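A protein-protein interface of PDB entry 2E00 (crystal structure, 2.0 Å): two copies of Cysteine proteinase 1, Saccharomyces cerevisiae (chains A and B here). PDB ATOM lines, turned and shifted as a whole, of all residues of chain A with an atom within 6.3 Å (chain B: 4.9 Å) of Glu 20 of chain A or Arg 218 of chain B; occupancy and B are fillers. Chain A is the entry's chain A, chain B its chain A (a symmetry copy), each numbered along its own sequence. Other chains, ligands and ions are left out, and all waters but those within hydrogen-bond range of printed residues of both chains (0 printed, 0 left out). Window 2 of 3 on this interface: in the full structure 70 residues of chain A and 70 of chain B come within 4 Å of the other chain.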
ATOM      1  N   ASN A  15      -7.083  16.029   6.257  1.00  0.00           N
ATOM      2  CA  ASN A  15      -7.335  16.713   7.521  1.00  0.00           C
ATOM      3  C   ASN A  15      -8.273  15.880   8.394  1.00  0.00           C
ATOM      4  O   ASN A  15      -8.171  15.900   9.623  1.00  0.00           O
ATOM      5  CB  ASN A  15      -7.878  18.122   7.295  1.00  0.00           C
ATOM      6  CG  ASN A  15      -6.774  19.121   7.004  1.00  0.00           C
ATOM      7  OD1 ASN A  15      -6.160  19.665   7.925  1.00  0.00           O
ATOM      8  ND2 ASN A  15      -6.501  19.352   5.724  1.00  0.00           N
ATOM      9  N   SER A  16      -9.153  15.113   7.756  1.00  0.00           N
ATOM     10  CA  SER A  16     -10.069  14.250   8.497  1.00  0.00           C
ATOM     11  C   SER A  16      -9.260  13.089   9.091  1.00  0.00           C
ATOM     12  O   SER A  16      -9.431  12.722  10.260  1.00  0.00           O
ATOM     13  CB  SER A  16     -11.174  13.722   7.575  1.00  0.00           C
ATOM     14  OG  SER A  16     -12.031  14.778   7.162  1.00  0.00           O
ATOM     15  N   TRP A  17      -8.373  12.520   8.279  1.00  0.00           N
ATOM     16  CA  TRP A  17      -7.519  11.431   8.729  1.00  0.00           C
ATOM     17  C   TRP A  17      -6.649  11.923   9.881  1.00  0.00           C
ATOM     18  O   TRP A  17      -6.441  11.207  10.862  1.00  0.00           O
ATOM     19  CB  TRP A  17      -6.620  10.935   7.589  1.00  0.00           C
ATOM     20  CG  TRP A  17      -7.333  10.121   6.557  1.00  0.00           C
ATOM     21  CD1 TRP A  17      -8.487   9.398   6.727  1.00  0.00           C
ATOM     22  CD2 TRP A  17      -6.941   9.933   5.192  1.00  0.00           C
ATOM     23  NE1 TRP A  17      -8.831   8.773   5.551  1.00  0.00           N
ATOM     24  CE2 TRP A  17      -7.901   9.083   4.594  1.00  0.00           C
ATOM     25  CE3 TRP A  17      -5.871  10.400   4.416  1.00  0.00           C
ATOM     26  CZ2 TRP A  17      -7.822   8.691   3.255  1.00  0.00           C
ATOM     27  CZ3 TRP A  17      -5.792  10.010   3.083  1.00  0.00           C
ATOM     28  CH2 TRP A  17      -6.762   9.162   2.517  1.00  0.00           C
ATOM     29  N   ASN A  18      -6.160  13.154   9.762  1.00  0.00           N
ATOM     30  CA  ASN A  18      -5.310  13.731  10.799  1.00  0.00           C
ATOM     31  C   ASN A  18      -6.030  13.770  12.143  1.00  0.00           C
ATOM     32  O   ASN A  18      -5.451  13.404  13.170  1.00  0.00           O
ATOM     33  CB  ASN A  18      -4.849  15.138  10.418  1.00  0.00           C
ATOM     34  CG  ASN A  18      -3.839  15.698  11.396  1.00  0.00           C
ATOM     35  OD1 ASN A  18      -2.764  15.125  11.586  1.00  0.00           O
ATOM     36  ND2 ASN A  18      -4.185  16.807  12.043  1.00  0.00           N
ATOM     37  N   LYS A  19      -7.287  14.216  12.133  1.00  0.00           N
ATOM     38  CA  LYS A  19      -8.077  14.277  13.361  1.00  0.00           C
ATOM     39  C   LYS A  19      -8.185  12.881  13.970  1.00  0.00           C
ATOM     40  O   LYS A  19      -7.992  12.702  15.182  1.00  0.00           O
ATOM     41  CB  LYS A  19      -9.479  14.832  13.087  1.00  0.00           C
ATOM     42  CG  LYS A  19     -10.312  15.003  14.349  1.00  0.00           C
ATOM     43  CD  LYS A  19     -11.710  15.532  14.038  1.00  0.00           C
ATOM     44  CE  LYS A  19     -12.529  15.694  15.311  1.00  0.00           C
ATOM     45  NZ  LYS A  19     -13.912  16.158  15.013  1.00  0.00           N
ATOM     46  N   GLU A  20      -8.465  11.887  13.129  1.00  0.00           N
ATOM     47  CA  GLU A  20      -8.573  10.512  13.606  1.00  0.00           C
ATOM     48  C   GLU A  20      -7.263  10.039  14.247  1.00  0.00           C
ATOM     49  O   GLU A  20      -7.268   9.505  15.359  1.00  0.00           O
ATOM     50  CB  GLU A  20      -8.954   9.563  12.471  1.00  0.00           C
ATOM     51  CG  GLU A  20      -9.049   8.111  12.925  1.00  0.00           C
ATOM     52  CD  GLU A  20      -9.574   7.167  11.855  1.00  0.00           C
ATOM     53  OE1 GLU A  20     -10.322   7.606  10.957  1.00  0.00           O
ATOM     54  OE2 GLU A  20      -9.256   5.964  11.931  1.00  0.00           O
ATOM     55  N   PHE A  21      -6.150  10.233  13.544  1.00  0.00           N
ATOM     56  CA  PHE A  21      -4.843   9.820  14.056  1.00  0.00           C
ATOM     57  C   PHE A  21      -4.490  10.514  15.373  1.00  0.00           C
ATOM     58  O   PHE A  21      -3.992   9.874  16.303  1.00  0.00           O
ATOM     59  CB  PHE A  21      -3.748  10.077  13.011  1.00  0.00           C
ATOM     60  CG  PHE A  21      -3.925   9.295  11.735  1.00  0.00           C
ATOM     61  CD1 PHE A  21      -4.496   8.026  11.750  1.00  0.00           C
ATOM     62  CD2 PHE A  21      -3.525   9.833  10.515  1.00  0.00           C
ATOM     63  CE1 PHE A  21      -4.672   7.306  10.569  1.00  0.00           C
ATOM     64  CE2 PHE A  21      -3.696   9.121   9.331  1.00  0.00           C
ATOM     65  CZ  PHE A  21      -4.270   7.859   9.357  1.00  0.00           C
ATOM     66  N   GLN A  22      -4.790  11.809  15.468  1.00  0.00           N
ATOM     67  CA  GLN A  22      -4.502  12.582  16.677  1.00  0.00           C
ATOM     68  C   GLN A  22      -5.285  12.132  17.912  1.00  0.00           C
ATOM     69  O   GLN A  22      -4.913  12.471  19.036  1.00  0.00           O
ATOM     70  CB  GLN A  22      -4.722  14.079  16.434  1.00  0.00           C
ATOM     71  CG  GLN A  22      -3.618  14.764  15.626  1.00  0.00           C
ATOM     72  CD  GLN A  22      -2.274  14.786  16.346  1.00  0.00           C
ATOM     73  OE1 GLN A  22      -1.222  14.584  15.732  1.00  0.00           O
ATOM     74  NE2 GLN A  22      -2.304  15.048  17.650  1.00  0.00           N
ATOM     75  N   SER A  23      -6.355  11.367  17.701  1.00  0.00           N
ATOM     76  CA  SER A  23      -7.177  10.864  18.802  1.00  0.00           C
ATOM     77  C   SER A  23      -6.580   9.586  19.395  1.00  0.00           C
ATOM     78  O   SER A  23      -7.073   9.063  20.393  1.00  0.00           O
ATOM     79  CB  SER A  23      -8.613  10.601  18.329  1.00  0.00           C
ATOM     80  OG  SER A  23      -8.706   9.411  17.562  1.00  0.00           O
ATOM     81  N   ASP A  24      -5.550   9.059  18.740  1.00  0.00           N
ATOM     82  CA  ASP A  24      -4.881   7.855  19.210  1.00  0.00           C
ATOM     83  C   ASP A  24      -3.625   8.247  19.993  1.00  0.00           C
ATOM     84  O   ASP A  24      -2.757   8.951  19.477  1.00  0.00           O
ATOM     85  CB  ASP A  24      -4.517   6.955  18.026  1.00  0.00           C
ATOM     86  CG  ASP A  24      -3.849   5.667  18.461  1.00  0.00           C
ATOM     87  OD1 ASP A  24      -4.560   4.767  18.959  1.00  0.00           O
ATOM     88  OD2 ASP A  24      -2.613   5.561  18.311  1.00  0.00           O
ATOM     89  N   GLU B 214      -6.878   4.169  -1.950  1.00  0.00           N
ATOM     90  CA  GLU B 214      -7.221   5.092  -0.875  1.00  0.00           C
ATOM     91  C   GLU B 214      -6.578   4.666   0.441  1.00  0.00           C
ATOM     92  O   GLU B 214      -6.111   5.508   1.210  1.00  0.00           O
ATOM     93  CB  GLU B 214      -8.732   5.223  -0.695  1.00  0.00           C
ATOM     94  CG  GLU B 214      -9.090   6.319   0.302  1.00  0.00           C
ATOM     95  CD  GLU B 214     -10.578   6.528   0.445  1.00  0.00           C
ATOM     96  OE1 GLU B 214     -11.266   5.604   0.933  1.00  0.00           O
ATOM     97  OE2 GLU B 214     -11.054   7.623   0.076  1.00  0.00           O
ATOM     98  N   GLN B 215      -6.569   3.365   0.706  1.00  0.00           N
ATOM     99  CA  GLN B 215      -5.953   2.855   1.923  1.00  0.00           C
ATOM    100  C   GLN B 215      -4.463   3.202   1.905  1.00  0.00           C
ATOM    101  O   GLN B 215      -3.886   3.526   2.941  1.00  0.00           O
ATOM    102  CB  GLN B 215      -6.134   1.338   2.035  1.00  0.00           C
ATOM    103  CG  GLN B 215      -7.575   0.895   2.246  1.00  0.00           C
ATOM    104  CD  GLN B 215      -7.739  -0.617   2.222  1.00  0.00           C
ATOM    105  OE1 GLN B 215      -6.906  -1.339   1.664  1.00  0.00           O
ATOM    106  NE2 GLN B 215      -8.821  -1.103   2.821  1.00  0.00           N
ATOM    107  N   MET B 216      -3.857   3.162   0.718  1.00  0.00           N
ATOM    108  CA  MET B 216      -2.443   3.481   0.571  1.00  0.00           C
ATOM    109  C   MET B 216      -2.175   4.957   0.855  1.00  0.00           C
ATOM    110  O   MET B 216      -1.222   5.282   1.560  1.00  0.00           O
ATOM    111  CB  MET B 216      -1.929   3.059  -0.810  1.00  0.00           C
ATOM    112  CG  MET B 216      -1.846   1.539  -0.968  1.00  0.00           C
ATOM    113  SD  MET B 216      -1.428   0.998  -2.630  1.00  0.00           S
ATOM    114  CE  MET B 216      -1.183  -0.769  -2.353  1.00  0.00           C
ATOM    115  N   GLN B 217      -3.033   5.843   0.347  1.00  0.00           N
ATOM    116  CA  GLN B 217      -2.882   7.278   0.602  1.00  0.00           C
ATOM    117  C   GLN B 217      -2.935   7.514   2.108  1.00  0.00           C
ATOM    118  O   GLN B 217      -2.143   8.270   2.658  1.00  0.00           O
ATOM    119  CB  GLN B 217      -4.028   8.085  -0.011  1.00  0.00           C
ATOM    120  CG  GLN B 217      -4.004   8.308  -1.507  1.00  0.00           C
ATOM    121  CD  GLN B 217      -5.068   9.309  -1.937  1.00  0.00           C
ATOM    122  OE1 GLN B 217      -6.005   9.595  -1.188  1.00  0.00           O
ATOM    123  NE2 GLN B 217      -4.916   9.860  -3.132  1.00  0.00           N
ATOM    124  N   ARG B 218      -3.896   6.860   2.757  1.00  0.00           N
ATOM    125  CA  ARG B 218      -4.102   6.982   4.197  1.00  0.00           C
ATOM    126  C   ARG B 218      -2.849   6.580   4.966  1.00  0.00           C
ATOM    127  O   ARG B 218      -2.434   7.280   5.884  1.00  0.00           O
ATOM    128  CB  ARG B 218      -5.289   6.121   4.626  1.00  0.00           C
ATOM    129  CG  ARG B 218      -5.714   6.277   6.082  1.00  0.00           C
ATOM    130  CD  ARG B 218      -7.065   5.605   6.289  1.00  0.00           C
ATOM    131  NE  ARG B 218      -7.581   5.771   7.645  1.00  0.00           N
ATOM    132  CZ  ARG B 218      -7.166   5.067   8.694  1.00  0.00           C
ATOM    133  NH1 ARG B 218      -6.222   4.146   8.548  1.00  0.00           N
ATOM    134  NH2 ARG B 218      -7.706   5.266   9.884  1.00  0.00           N
ATOM    135  N   GLU B 219      -2.246   5.462   4.571  1.00  0.00           N
ATOM    136  CA  GLU B 219      -1.041   4.981   5.226  1.00  0.00           C
ATOM    137  C   GLU B 219       0.146   5.918   4.978  1.00  0.00           C
ATOM    138  O   GLU B 219       0.965   6.144   5.871  1.00  0.00           O
ATOM    139  CB  GLU B 219      -0.715   3.564   4.758  1.00  0.00           C
ATOM    140  CG  GLU B 219       0.335   2.860   5.610  1.00  0.00           C
ATOM    141  CD  GLU B 219      -0.159   2.468   7.006  1.00  0.00           C
ATOM    142  OE1 GLU B 219      -1.145   3.052   7.523  1.00  0.00           O
ATOM    143  OE2 GLU B 219       0.458   1.559   7.597  1.00  0.00           O
ATOM    144  N   ILE B 220       0.243   6.448   3.761  1.00  0.00           N
ATOM    145  CA  ILE B 220       1.318   7.380   3.424  1.00  0.00           C
ATOM    146  C   ILE B 220       1.156   8.641   4.271  1.00  0.00           C
ATOM    147  O   ILE B 220       2.121   9.128   4.873  1.00  0.00           O
ATOM    148  CB  ILE B 220       1.287   7.770   1.931  1.00  0.00           C
ATOM    149  CG1 ILE B 220       1.637   6.560   1.062  1.00  0.00           C
ATOM    150  CG2 ILE B 220       2.266   8.907   1.656  1.00  0.00           C
ATOM    151  CD1 ILE B 220       1.405   6.805  -0.425  1.00  0.00           C
ATOM    152  N   PHE B 221      -0.069   9.163   4.329  1.00  0.00           N
ATOM    153  CA  PHE B 221      -0.319  10.355   5.122  1.00  0.00           C
ATOM    154  C   PHE B 221      -0.026  10.099   6.596  1.00  0.00           C
ATOM    155  O   PHE B 221       0.593  10.932   7.268  1.00  0.00           O
ATOM    156  CB  PHE B 221      -1.758  10.873   4.973  1.00  0.00           C
ATOM    157  CG  PHE B 221      -2.034  12.083   5.824  1.00  0.00           C
ATOM    158  CD1 PHE B 221      -1.497  13.323   5.480  1.00  0.00           C
ATOM    159  CD2 PHE B 221      -2.727  11.963   7.023  1.00  0.00           C
ATOM    160  CE1 PHE B 221      -1.637  14.420   6.322  1.00  0.00           C
ATOM    161  CE2 PHE B 221      -2.873  13.059   7.876  1.00  0.00           C
ATOM    162  CZ  PHE B 221      -2.325  14.287   7.526  1.00  0.00           C
ATOM    163  N   ARG B 222      -0.474   8.951   7.094  1.00  0.00           N
ATOM    164  CA  ARG B 222      -0.260   8.595   8.494  1.00  0.00           C
ATOM    165  C   ARG B 222       1.229   8.586   8.831  1.00  0.00           C
ATOM    166  O   ARG B 222       1.644   9.180   9.825  1.00  0.00           O
ATOM    167  CB  ARG B 222      -0.861   7.225   8.793  1.00  0.00           C
ATOM    168  CG  ARG B 222      -0.752   6.806  10.243  1.00  0.00           C
ATOM    169  CD  ARG B 222      -1.087   5.330  10.389  1.00  0.00           C
ATOM    170  NE  ARG B 222      -0.153   4.686  11.302  1.00  0.00           N
ATOM    171  CZ  ARG B 222       0.806   3.847  10.933  1.00  0.00           C
ATOM    172  NH1 ARG B 222       0.973   3.519   9.663  1.00  0.00           N
ATOM    173  NH2 ARG B 222       1.614   3.348  11.844  1.00  0.00           N
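Glu 20 of chain A touches just one residue of chain B: Arg 218. Printed residues of chain B within 4 Å of Phe 21 of chain A: Arg 218 (3.7 Å), Phe 221 (3.8 Å) and Arg 222 (3.5 Å). Of the printed residues of chain A, Gln 217 of chain B touches Trp 17 (3.8 Å). Arg 218 of chain B touches just these residues of chain A: Trp 17, Glu 20 and Phe 21.
No position is printed for both chains.
NH1 of Arg 222 of chain B is in salt-bridge range of OE2 of Glu 219 of chain B, 2.9 Å away. The side-chain hydroxyl (OG) of Ser 23 of chain A sits at hydrogen-bond distance from the backbone carbonyl oxygen (O) of Glu 20 of chain A (2.6 Å).
Trp 17 of chain A touches Glu 214 of chain B (CH2 to O, 3.9 Å). Gln 217 of chain B touches Trp 17 of chain A. Trp 17 of chain A touches Arg 218 of chain B. N of Asn 18 of chain A touches CE2 of Phe 221 of chain B, 3.8 Å away. CE1 of Phe 21 of chain A touches NH2 of Arg 218 of chain B (3.7 Å). Phe 21 of chain A touches Phe 221 of chain B. Arg 222 of chain B touches Phe 21 of chain A (CB to CE2, 3.5 Å).
Along chain A the printed residues that touch a printed residue of chain B span positions 17 to 21. Of the 9 printed residues of chain B, 5 touch a printed residue of chain A. Hydrophobic or aromatic side chains of chain B within 4 Å of the printed part of chain A: Phe 221.
NH2 of Arg 218 of chain B is in salt-bridge range of OE2 of Glu 20 of chain A (2.7 Å).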
